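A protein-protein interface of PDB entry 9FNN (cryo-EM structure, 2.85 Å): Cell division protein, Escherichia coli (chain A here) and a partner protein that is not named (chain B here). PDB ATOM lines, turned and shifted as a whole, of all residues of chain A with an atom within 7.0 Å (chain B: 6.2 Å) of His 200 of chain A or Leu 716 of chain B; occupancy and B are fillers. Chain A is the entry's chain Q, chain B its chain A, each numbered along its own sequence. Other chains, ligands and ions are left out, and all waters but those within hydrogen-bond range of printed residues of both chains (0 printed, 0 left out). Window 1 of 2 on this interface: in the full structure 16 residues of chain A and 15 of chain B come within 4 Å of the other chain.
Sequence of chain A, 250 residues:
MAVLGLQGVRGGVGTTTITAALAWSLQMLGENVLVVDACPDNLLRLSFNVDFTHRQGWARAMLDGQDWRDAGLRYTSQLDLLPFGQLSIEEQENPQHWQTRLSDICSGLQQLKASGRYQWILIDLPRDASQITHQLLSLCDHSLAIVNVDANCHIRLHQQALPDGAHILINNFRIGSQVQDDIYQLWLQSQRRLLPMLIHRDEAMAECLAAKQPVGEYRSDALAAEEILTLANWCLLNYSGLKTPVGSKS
O of Gly 714 of chain B is in hydrogen-bond range of N of Glu 203 of chain A (2.8 Å).
N of Leu 716 of chain B lies within hydrogen-bond range of OD1 of Asp 202 of chain A (2.9 Å).
The backbone NH (N) of Leu 223 of chain A lies within hydrogen-bond range of the backbone carbonyl oxygen (O) of Leu 716 of chain B, 3.0 Å away.
A ring nitrogen (NE2) of His 200 of chain A lies within hydrogen-bond range of the side-chain carboxylate of Glu 755 of chain B (2.5 Å).
The backbone carbonyl oxygen (O) of Gly 714 of chain B lies close to the side-chain carboxylate (OD1) of Asp 202 of chain A.
Hydrophobic or aromatic side chains of chain B within 4 Å of the printed part of chain A: Ala 708, Ala 710, His 715, Leu 716, Phe 717 and Leu 748.
Along chain B the printed residues that touch a printed residue of chain A span positions 708 to 755.
Printed residues of chain A that touch a printed residue of chain B: Phe 173, Ile 175, His 200, Arg 201, Asp 202, Glu 203, Arg 219, Asp 221, Ala 222 and Leu 223.
Among the printed residues, 17 pairs touch across the chains.
Among the printed residues, no Asp or Glu carboxylate lies within 4 Å of a Lys or Arg side-chain nitrogen of the other chain.
Among the printed residues, merely in contact across the chains: Arg 219 of chain A with Phe 717 of chain B, Asp 202 of chain A with His 715 of chain B, Asp 221 of chain A with Phe 717 of chain B, Glu 203 of chain A with His 715 of chain B, His 200 of chain A with Leu 716 of chain B, Leu 223 of chain A with Ala 708 of chain B, Ala 222 of chain A with Leu 716 of chain B, Ile 175 of chain A with Ala 710 of chain B, Leu 223 of chain A with Ser 718 of chain B, Ile 175 of chain A with Leu 748 of chain B, Arg 201 of chain A with Leu 716 of chain B and Phe 173 of chain A with Glu 755 of chain B.
His 200 of chain A touches two residues of chain B.
Leu 716 of chain B touches just these residues of chain A: His 200 (3.6 Å), Arg 201 (3.9 Å), Asp 202 (2.9 Å), Ala 222 (3.7 Å) and Leu 223 (3.0 Å).
Of the printed residues of chain A, Ala 708 of chain B touches Leu 223 (3.6 Å).
Of the printed residues of chain B, Phe 173 of chain A touches Glu 755.
Of the printed residues of chain B, Arg 219 of chain A touches Phe 717.
Of the printed residues of chain A, His 715 of chain B touches Asp 202 and Glu 203.
Printed residues of chain A within 4 Å of Gly 714 of chain B: Asp 202 and Glu 203.
Ala 204 of chain A touches none of the printed residues of chain B.
The nearest residue of chain B that does not touch His 200 of chain A is Leu 748 of chain B (4.03 Å).
The nearest printed residue of chain B that does not touch Glu 203 of chain A is Leu 716 of chain B (5.2 Å).
The backbone NH of Leu 748 of chain B lies within hydrogen-bond range of the backbone carbonyl oxygen of Ala 708 of chain B (2.8 Å).
The backbone NH of Ile 709 of chain B sits at hydrogen-bond distance from the backbone carbonyl oxygen of Phe 717 of chain B.
The backbone NH (N) of Phe 173 of chain A sits at hydrogen-bond distance from the backbone carbonyl oxygen (O) of Ile 199 of chain A.
OE2 of Glu 227 of chain A is in hydrogen-bond range of ND1 of His 200 of chain A (3.0 Å).
The guanidinium group (NH2) of Arg 201 of chain A is in salt-bridge range of the side-chain carboxylate (OE1) of Glu 203 of chain A, at 3.5 Å.
The guanidinium group of Arg 219 of chain A is in salt-bridge range of the side-chain carboxylate of Asp 221 of chain A (3.2 Å).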
ATOM      1  N   ILE A 170      -1.527 -10.984 -27.315  1.00  0.00           N
ATOM      2  CA  ILE A 170      -2.486 -10.603 -26.289  1.00  0.00           C
ATOM      3  C   ILE A 170      -2.753  -9.111 -26.401  1.00  0.00           C
ATOM      4  O   ILE A 170      -1.823  -8.299 -26.359  1.00  0.00           O
ATOM      5  CB  ILE A 170      -1.979 -10.969 -24.887  1.00  0.00           C
ATOM      6  CG1 ILE A 170      -1.987 -12.483 -24.701  1.00  0.00           C
ATOM      7  CG2 ILE A 170      -2.822 -10.293 -23.827  1.00  0.00           C
ATOM      8  CD1 ILE A 170      -1.445 -12.932 -23.377  1.00  0.00           C
ATOM      9  N   ASN A 171      -4.024  -8.751 -26.544  1.00  0.00           N
ATOM     10  CA  ASN A 171      -4.469  -7.370 -26.558  1.00  0.00           C
ATOM     11  C   ASN A 171      -5.369  -7.126 -25.354  1.00  0.00           C
ATOM     12  O   ASN A 171      -5.884  -8.066 -24.742  1.00  0.00           O
ATOM     13  CB  ASN A 171      -5.214  -7.043 -27.857  1.00  0.00           C
ATOM     14  CG  ASN A 171      -5.444  -5.562 -28.043  1.00  0.00           C
ATOM     15  OD1 ASN A 171      -4.728  -4.738 -27.483  1.00  0.00           O
ATOM     16  ND2 ASN A 171      -6.449  -5.216 -28.830  1.00  0.00           N
ATOM     17  N   ASN A 172      -5.546  -5.851 -25.015  1.00  0.00           N
ATOM     18  CA  ASN A 172      -6.435  -5.430 -23.931  1.00  0.00           C
ATOM     19  C   ASN A 172      -6.050  -6.074 -22.603  1.00  0.00           C
ATOM     20  O   ASN A 172      -6.893  -6.584 -21.866  1.00  0.00           O
ATOM     21  CB  ASN A 172      -7.897  -5.725 -24.270  1.00  0.00           C
ATOM     22  CG  ASN A 172      -8.512  -4.674 -25.160  1.00  0.00           C
ATOM     23  OD1 ASN A 172      -8.238  -3.484 -25.014  1.00  0.00           O
ATOM     24  ND2 ASN A 172      -9.350  -5.105 -26.090  1.00  0.00           N
ATOM     25  N   PHE A 173      -4.759  -6.047 -22.296  1.00  0.00           N
ATOM     26  CA  PHE A 173      -4.302  -6.509 -20.994  1.00  0.00           C
ATOM     27  C   PHE A 173      -4.634  -5.453 -19.950  1.00  0.00           C
ATOM     28  O   PHE A 173      -4.167  -4.314 -20.039  1.00  0.00           O
ATOM     29  CB  PHE A 173      -2.804  -6.795 -21.028  1.00  0.00           C
ATOM     30  CG  PHE A 173      -2.361  -7.799 -20.013  1.00  0.00           C
ATOM     31  CD1 PHE A 173      -2.642  -9.139 -20.184  1.00  0.00           C
ATOM     32  CD2 PHE A 173      -1.661  -7.407 -18.891  1.00  0.00           C
ATOM     33  CE1 PHE A 173      -2.240 -10.064 -19.253  1.00  0.00           C
ATOM     34  CE2 PHE A 173      -1.255  -8.331 -17.958  1.00  0.00           C
ATOM     35  CZ  PHE A 173      -1.544  -9.660 -18.139  1.00  0.00           C
ATOM     36  N   ARG A 174      -5.437  -5.830 -18.962  1.00  0.00           N
ATOM     37  CA  ARG A 174      -6.023  -4.883 -18.031  1.00  0.00           C
ATOM     38  C   ARG A 174      -5.221  -4.819 -16.735  1.00  0.00           C
ATOM     39  O   ARG A 174      -4.178  -5.454 -16.576  1.00  0.00           O
ATOM     40  CB  ARG A 174      -7.479  -5.250 -17.757  1.00  0.00           C
ATOM     41  CG  ARG A 174      -8.310  -5.321 -19.011  1.00  0.00           C
ATOM     42  CD  ARG A 174      -9.768  -5.540 -18.718  1.00  0.00           C
ATOM     43  NE  ARG A 174     -10.523  -5.697 -19.954  1.00  0.00           N
ATOM     44  CZ  ARG A 174     -11.017  -4.691 -20.661  1.00  0.00           C
ATOM     45  NH1 ARG A 174     -10.873  -3.436 -20.270  1.00  0.00           N
ATOM     46  NH2 ARG A 174     -11.671  -4.951 -21.790  1.00  0.00           N
ATOM     47  N   ILE A 175      -5.731  -4.030 -15.797  1.00  0.00           N
ATOM     48  CA  ILE A 175      -5.068  -3.739 -14.533  1.00  0.00           C
ATOM     49  C   ILE A 175      -5.977  -4.188 -13.400  1.00  0.00           C
ATOM     50  O   ILE A 175      -7.163  -3.840 -13.374  1.00  0.00           O
ATOM     51  CB  ILE A 175      -4.742  -2.240 -14.410  1.00  0.00           C
ATOM     52  CG1 ILE A 175      -3.591  -1.865 -15.339  1.00  0.00           C
ATOM     53  CG2 ILE A 175      -4.437  -1.870 -12.973  1.00  0.00           C
ATOM     54  CD1 ILE A 175      -3.282  -0.393 -15.355  1.00  0.00           C
ATOM     55  N   LEU A 198       2.920  -8.161 -24.945  1.00  0.00           N
ATOM     56  CA  LEU A 198       1.475  -8.024 -24.888  1.00  0.00           C
ATOM     57  C   LEU A 198       1.096  -6.553 -24.935  1.00  0.00           C
ATOM     58  O   LEU A 198       1.819  -5.692 -24.427  1.00  0.00           O
ATOM     59  CB  LEU A 198       0.895  -8.688 -23.630  1.00  0.00           C
ATOM     60  CG  LEU A 198       1.545  -8.435 -22.269  1.00  0.00           C
ATOM     61  CD1 LEU A 198       1.083  -7.129 -21.659  1.00  0.00           C
ATOM     62  CD2 LEU A 198       1.245  -9.586 -21.334  1.00  0.00           C
ATOM     63  N   ILE A 199      -0.041  -6.273 -25.558  1.00  0.00           N
ATOM     64  CA  ILE A 199      -0.582  -4.923 -25.629  1.00  0.00           C
ATOM     65  C   ILE A 199      -1.480  -4.705 -24.423  1.00  0.00           C
ATOM     66  O   ILE A 199      -2.216  -5.607 -24.010  1.00  0.00           O
ATOM     67  CB  ILE A 199      -1.351  -4.702 -26.944  1.00  0.00           C
ATOM     68  CG1 ILE A 199      -0.591  -5.296 -28.126  1.00  0.00           C
ATOM     69  CG2 ILE A 199      -1.592  -3.225 -27.176  1.00  0.00           C
ATOM     70  CD1 ILE A 199       0.726  -4.635 -28.396  1.00  0.00           C
ATOM     71  N   HIS A 200      -1.423  -3.511 -23.852  1.00  0.00           N
ATOM     72  CA  HIS A 200      -2.214  -3.168 -22.683  1.00  0.00           C
ATOM     73  C   HIS A 200      -3.513  -2.482 -23.084  1.00  0.00           C
ATOM     74  O   HIS A 200      -3.705  -2.059 -24.225  1.00  0.00           O
ATOM     75  CB  HIS A 200      -1.421  -2.267 -21.739  1.00  0.00           C
ATOM     76  CG  HIS A 200      -0.614  -3.011 -20.726  1.00  0.00           C
ATOM     77  ND1 HIS A 200       0.608  -3.575 -21.018  1.00  0.00           N
ATOM     78  CD2 HIS A 200      -0.852  -3.281 -19.423  1.00  0.00           C
ATOM     79  CE1 HIS A 200       1.088  -4.161 -19.936  1.00  0.00           C
ATOM     80  NE2 HIS A 200       0.220  -3.999 -18.955  1.00  0.00           N
ATOM     81  N   ARG A 201      -4.415  -2.378 -22.112  1.00  0.00           N
ATOM     82  CA  ARG A 201      -5.668  -1.646 -22.267  1.00  0.00           C
ATOM     83  C   ARG A 201      -5.354  -0.167 -22.091  1.00  0.00           C
ATOM     84  O   ARG A 201      -5.290   0.355 -20.977  1.00  0.00           O
ATOM     85  CB  ARG A 201      -6.702  -2.139 -21.263  1.00  0.00           C
ATOM     86  CG  ARG A 201      -7.965  -1.310 -21.183  1.00  0.00           C
ATOM     87  CD  ARG A 201      -8.748  -1.344 -22.469  1.00  0.00           C
ATOM     88  NE  ARG A 201      -9.825  -0.362 -22.459  1.00  0.00           N
ATOM     89  CZ  ARG A 201      -9.660   0.927 -22.721  1.00  0.00           C
ATOM     90  NH1 ARG A 201      -8.471   1.426 -23.014  1.00  0.00           N
ATOM     91  NH2 ARG A 201     -10.713   1.736 -22.689  1.00  0.00           N
ATOM     92  N   ASP A 202      -5.139   0.514 -23.211  1.00  0.00           N
ATOM     93  CA  ASP A 202      -4.727   1.908 -23.225  1.00  0.00           C
ATOM     94  C   ASP A 202      -5.792   2.749 -23.911  1.00  0.00           C
ATOM     95  O   ASP A 202      -6.313   2.368 -24.963  1.00  0.00           O
ATOM     96  CB  ASP A 202      -3.381   2.071 -23.935  1.00  0.00           C
ATOM     97  CG  ASP A 202      -2.782   3.445 -23.743  1.00  0.00           C
ATOM     98  OD1 ASP A 202      -3.344   4.242 -22.964  1.00  0.00           O
ATOM     99  OD2 ASP A 202      -1.743   3.729 -24.371  1.00  0.00           O
ATOM    100  N   GLU A 203      -6.112   3.893 -23.305  1.00  0.00           N
ATOM    101  CA  GLU A 203      -7.119   4.787 -23.864  1.00  0.00           C
ATOM    102  C   GLU A 203      -6.711   5.333 -25.223  1.00  0.00           C
ATOM    103  O   GLU A 203      -7.579   5.737 -26.005  1.00  0.00           O
ATOM    104  CB  GLU A 203      -7.383   5.940 -22.897  1.00  0.00           C
ATOM    105  CG  GLU A 203      -8.681   6.685 -23.141  1.00  0.00           C
ATOM    106  CD  GLU A 203      -9.890   5.937 -22.623  1.00  0.00           C
ATOM    107  OE1 GLU A 203      -9.710   4.967 -21.858  1.00  0.00           O
ATOM    108  OE2 GLU A 203     -11.023   6.321 -22.979  1.00  0.00           O
ATOM    109  N   ALA A 204      -5.412   5.349 -25.523  1.00  0.00           N
ATOM    110  CA  ALA A 204      -4.958   5.835 -26.817  1.00  0.00           C
ATOM    111  C   ALA A 204      -5.494   4.971 -27.950  1.00  0.00           C
ATOM    112  O   ALA A 204      -5.842   5.483 -29.018  1.00  0.00           O
ATOM    113  CB  ALA A 204      -3.434   5.884 -26.852  1.00  0.00           C
ATOM    114  N   MET A 205      -5.564   3.657 -27.737  1.00  0.00           N
ATOM    115  CA  MET A 205      -6.115   2.772 -28.758  1.00  0.00           C
ATOM    116  C   MET A 205      -7.600   3.023 -28.965  1.00  0.00           C
ATOM    117  O   MET A 205      -8.103   2.921 -30.089  1.00  0.00           O
ATOM    118  CB  MET A 205      -5.869   1.316 -28.378  1.00  0.00           C
ATOM    119  CG  MET A 205      -4.410   0.948 -28.249  1.00  0.00           C
ATOM    120  SD  MET A 205      -3.644   0.476 -29.805  1.00  0.00           S
ATOM    121  CE  MET A 205      -4.261  -1.191 -29.989  1.00  0.00           C
ATOM    122  N   ARG A 219      -0.697   9.215 -30.993  1.00  0.00           N
ATOM    123  CA  ARG A 219      -0.031   9.419 -29.708  1.00  0.00           C
ATOM    124  C   ARG A 219       1.201   8.520 -29.672  1.00  0.00           C
ATOM    125  O   ARG A 219       1.087   7.321 -29.405  1.00  0.00           O
ATOM    126  CB  ARG A 219      -0.975   9.120 -28.554  1.00  0.00           C
ATOM    127  CG  ARG A 219      -0.411   9.441 -27.192  1.00  0.00           C
ATOM    128  CD  ARG A 219      -1.094  10.646 -26.586  1.00  0.00           C
ATOM    129  NE  ARG A 219      -0.412  11.097 -25.380  1.00  0.00           N
ATOM    130  CZ  ARG A 219      -0.951  11.888 -24.464  1.00  0.00           C
ATOM    131  NH1 ARG A 219      -2.195  12.321 -24.570  1.00  0.00           N
ATOM    132  NH2 ARG A 219      -0.223  12.250 -23.412  1.00  0.00           N
ATOM    133  N   ASP A 221       3.749   8.671 -27.589  1.00  0.00           N
ATOM    134  CA  ASP A 221       4.230   8.390 -26.244  1.00  0.00           C
ATOM    135  C   ASP A 221       3.350   7.399 -25.497  1.00  0.00           C
ATOM    136  O   ASP A 221       3.657   7.064 -24.350  1.00  0.00           O
ATOM    137  CB  ASP A 221       4.343   9.688 -25.439  1.00  0.00           C
ATOM    138  CG  ASP A 221       3.125  10.575 -25.588  1.00  0.00           C
ATOM    139  OD1 ASP A 221       2.573  10.647 -26.706  1.00  0.00           O
ATOM    140  OD2 ASP A 221       2.717  11.201 -24.586  1.00  0.00           O
ATOM    141  N   ALA A 222       2.272   6.929 -26.115  1.00  0.00           N
ATOM    142  CA  ALA A 222       1.415   5.936 -25.490  1.00  0.00           C
ATOM    143  C   ALA A 222       2.131   4.597 -25.385  1.00  0.00           C
ATOM    144  O   ALA A 222       2.956   4.239 -26.229  1.00  0.00           O
ATOM    145  CB  ALA A 222       0.122   5.774 -26.284  1.00  0.00           C
ATOM    146  N   LEU A 223       1.809   3.854 -24.326  1.00  0.00           N
ATOM    147  CA  LEU A 223       2.427   2.550 -24.125  1.00  0.00           C
ATOM    148  C   LEU A 223       2.034   1.571 -25.218  1.00  0.00           C
ATOM    149  O   LEU A 223       2.839   0.712 -25.598  1.00  0.00           O
ATOM    150  CB  LEU A 223       2.045   1.997 -22.756  1.00  0.00           C
ATOM    151  CG  LEU A 223       2.710   0.691 -22.334  1.00  0.00           C
ATOM    152  CD1 LEU A 223       4.215   0.857 -22.262  1.00  0.00           C
ATOM    153  CD2 LEU A 223       2.157   0.230 -21.004  1.00  0.00           C
ATOM    154  N   ALA A 224       0.809   1.682 -25.733  1.00  0.00           N
ATOM    155  CA  ALA A 224       0.380   0.801 -26.809  1.00  0.00           C
ATOM    156  C   ALA A 224       1.214   1.016 -28.063  1.00  0.00           C
ATOM    157  O   ALA A 224       1.560   0.054 -28.757  1.00  0.00           O
ATOM    158  CB  ALA A 224      -1.101   1.019 -27.103  1.00  0.00           C
ATOM    159  N   GLU A 227       4.547  -0.679 -27.498  1.00  0.00           N
ATOM    160  CA  GLU A 227       4.433  -2.129 -27.593  1.00  0.00           C
ATOM    161  C   GLU A 227       4.215  -2.585 -29.030  1.00  0.00           C
ATOM    162  O   GLU A 227       4.720  -3.642 -29.426  1.00  0.00           O
ATOM    163  CB  GLU A 227       3.310  -2.621 -26.686  1.00  0.00           C
ATOM    164  CG  GLU A 227       3.645  -2.506 -25.212  1.00  0.00           C
ATOM    165  CD  GLU A 227       2.423  -2.560 -24.326  1.00  0.00           C
ATOM    166  OE1 GLU A 227       1.302  -2.397 -24.849  1.00  0.00           O
ATOM    167  OE2 GLU A 227       2.582  -2.764 -23.105  1.00  0.00           O
ATOM    168  N   ALA B 708       5.746   1.148 -16.347  1.00  0.00           N
ATOM    169  CA  ALA B 708       4.665   1.879 -16.985  1.00  0.00           C
ATOM    170  C   ALA B 708       3.850   2.580 -15.911  1.00  0.00           C
ATOM    171  O   ALA B 708       3.815   2.152 -14.756  1.00  0.00           O
ATOM    172  CB  ALA B 708       3.779   0.951 -17.820  1.00  0.00           C
ATOM    173  N   ILE B 709       3.191   3.666 -16.303  1.00  0.00           N
ATOM    174  CA  ILE B 709       2.361   4.452 -15.400  1.00  0.00           C
ATOM    175  C   ILE B 709       0.952   4.521 -15.966  1.00  0.00           C
ATOM    176  O   ILE B 709       0.763   4.695 -17.173  1.00  0.00           O
ATOM    177  CB  ILE B 709       2.926   5.871 -15.165  1.00  0.00           C
ATOM    178  CG1 ILE B 709       3.364   6.515 -16.485  1.00  0.00           C
ATOM    179  CG2 ILE B 709       4.053   5.838 -14.144  1.00  0.00           C
ATOM    180  CD1 ILE B 709       4.033   7.870 -16.327  1.00  0.00           C
ATOM    181  N   ALA B 710      -0.034   4.370 -15.087  1.00  0.00           N
ATOM    182  CA  ALA B 710      -1.440   4.397 -15.454  1.00  0.00           C
ATOM    183  C   ALA B 710      -2.105   5.593 -14.794  1.00  0.00           C
ATOM    184  O   ALA B 710      -1.963   5.797 -13.585  1.00  0.00           O
ATOM    185  CB  ALA B 710      -2.141   3.105 -15.033  1.00  0.00           C
ATOM    186  N   ARG B 711      -2.827   6.377 -15.583  1.00  0.00           N
ATOM    187  CA  ARG B 711      -3.570   7.517 -15.076  1.00  0.00           C
ATOM    188  C   ARG B 711      -5.031   7.142 -14.856  1.00  0.00           C
ATOM    189  O   ARG B 711      -5.490   6.065 -15.243  1.00  0.00           O
ATOM    190  CB  ARG B 711      -3.461   8.702 -16.034  1.00  0.00           C
ATOM    191  CG  ARG B 711      -2.084   9.322 -16.122  1.00  0.00           C
ATOM    192  CD  ARG B 711      -2.165  10.670 -16.801  1.00  0.00           C
ATOM    193  NE  ARG B 711      -2.824  10.579 -18.095  1.00  0.00           N
ATOM    194  CZ  ARG B 711      -3.288  11.619 -18.772  1.00  0.00           C
ATOM    195  NH1 ARG B 711      -3.192  12.849 -18.298  1.00  0.00           N
ATOM    196  NH2 ARG B 711      -3.874  11.418 -19.949  1.00  0.00           N
ATOM    197  N   GLY B 714      -7.223   6.548 -18.000  1.00  0.00           N
ATOM    198  CA  GLY B 714      -6.990   5.344 -18.760  1.00  0.00           C
ATOM    199  C   GLY B 714      -5.834   5.384 -19.732  1.00  0.00           C
ATOM    200  O   GLY B 714      -5.710   4.465 -20.549  1.00  0.00           O
ATOM    201  N   HIS B 715      -4.990   6.407 -19.675  1.00  0.00           N
ATOM    202  CA  HIS B 715      -3.829   6.494 -20.546  1.00  0.00           C
ATOM    203  C   HIS B 715      -2.620   5.884 -19.852  1.00  0.00           C
ATOM    204  O   HIS B 715      -2.373   6.154 -18.674  1.00  0.00           O
ATOM    205  CB  HIS B 715      -3.536   7.944 -20.925  1.00  0.00           C
ATOM    206  CG  HIS B 715      -4.520   8.530 -21.885  1.00  0.00           C
ATOM    207  ND1 HIS B 715      -5.826   8.797 -21.541  1.00  0.00           N
ATOM    208  CD2 HIS B 715      -4.386   8.911 -23.176  1.00  0.00           C
ATOM    209  CE1 HIS B 715      -6.455   9.314 -22.580  1.00  0.00           C
ATOM    210  NE2 HIS B 715      -5.604   9.392 -23.585  1.00  0.00           N
ATOM    211  N   LEU B 716      -1.875   5.063 -20.582  1.00  0.00           N
ATOM    212  CA  LEU B 716      -0.671   4.433 -20.066  1.00  0.00           C
ATOM    213  C   LEU B 716       0.543   4.974 -20.804  1.00  0.00           C
ATOM    214  O   LEU B 716       0.501   5.178 -22.020  1.00  0.00           O
ATOM    215  CB  LEU B 716      -0.724   2.909 -20.213  1.00  0.00           C
ATOM    216  CG  LEU B 716      -1.964   2.131 -19.774  1.00  0.00           C
ATOM    217  CD1 LEU B 716      -1.627   0.663 -19.642  1.00  0.00           C
ATOM    218  CD2 LEU B 716      -2.533   2.658 -18.484  1.00  0.00           C
ATOM    219  N   PHE B 717       1.622   5.205 -20.064  1.00  0.00           N
ATOM    220  CA  PHE B 717       2.864   5.694 -20.640  1.00  0.00           C
ATOM    221  C   PHE B 717       4.025   4.898 -20.069  1.00  0.00           C
ATOM    222  O   PHE B 717       3.988   4.479 -18.910  1.00  0.00           O
ATOM    223  CB  PHE B 717       3.063   7.187 -20.357  1.00  0.00           C
ATOM    224  CG  PHE B 717       1.871   8.027 -20.695  1.00  0.00           C
ATOM    225  CD1 PHE B 717       1.645   8.437 -21.993  1.00  0.00           C
ATOM    226  CD2 PHE B 717       0.973   8.404 -19.714  1.00  0.00           C
ATOM    227  CE1 PHE B 717       0.552   9.206 -22.306  1.00  0.00           C
ATOM    228  CE2 PHE B 717      -0.122   9.172 -20.025  1.00  0.00           C
ATOM    229  CZ  PHE B 717      -0.332   9.573 -21.321  1.00  0.00           C
ATOM    230  N   SER B 718       5.048   4.689 -20.887  1.00  0.00           N
ATOM    231  CA  SER B 718       6.228   3.969 -20.443  1.00  0.00           C
ATOM    232  C   SER B 718       7.132   4.876 -19.619  1.00  0.00           C
ATOM    233  O   SER B 718       7.160   6.096 -19.799  1.00  0.00           O
ATOM    234  CB  SER B 718       7.001   3.416 -21.634  1.00  0.00           C
ATOM    235  OG  SER B 718       7.526   4.467 -22.421  1.00  0.00           O
ATOM    236  N   LEU B 748       3.177   0.192 -12.860  1.00  0.00           N
ATOM    237  CA  LEU B 748       3.231  -1.177 -13.353  1.00  0.00           C
ATOM    238  C   LEU B 748       4.671  -1.673 -13.323  1.00  0.00           C
ATOM    239  O   LEU B 748       5.533  -1.136 -14.026  1.00  0.00           O
ATOM    240  CB  LEU B 748       2.664  -1.268 -14.767  1.00  0.00           C
ATOM    241  CG  LEU B 748       1.280  -0.660 -14.997  1.00  0.00           C
ATOM    242  CD1 LEU B 748       0.799  -0.936 -16.408  1.00  0.00           C
ATOM    243  CD2 LEU B 748       0.291  -1.185 -13.985  1.00  0.00           C
ATOM    244  N   GLU B 755       3.175  -8.955 -14.235  1.00  0.00           N
ATOM    245  CA  GLU B 755       3.081  -7.524 -13.996  1.00  0.00           C
ATOM    246  C   GLU B 755       2.290  -7.262 -12.725  1.00  0.00           C
ATOM    247  O   GLU B 755       1.276  -7.915 -12.466  1.00  0.00           O
ATOM    248  CB  GLU B 755       2.420  -6.824 -15.182  1.00  0.00           C
ATOM    249  CG  GLU B 755       2.620  -5.327 -15.219  1.00  0.00           C
ATOM    250  CD  GLU B 755       2.038  -4.706 -16.469  1.00  0.00           C
ATOM    251  OE1 GLU B 755       1.044  -5.248 -16.992  1.00  0.00           O
ATOM    252  OE2 GLU B 755       2.581  -3.682 -16.935  1.00  0.00           O
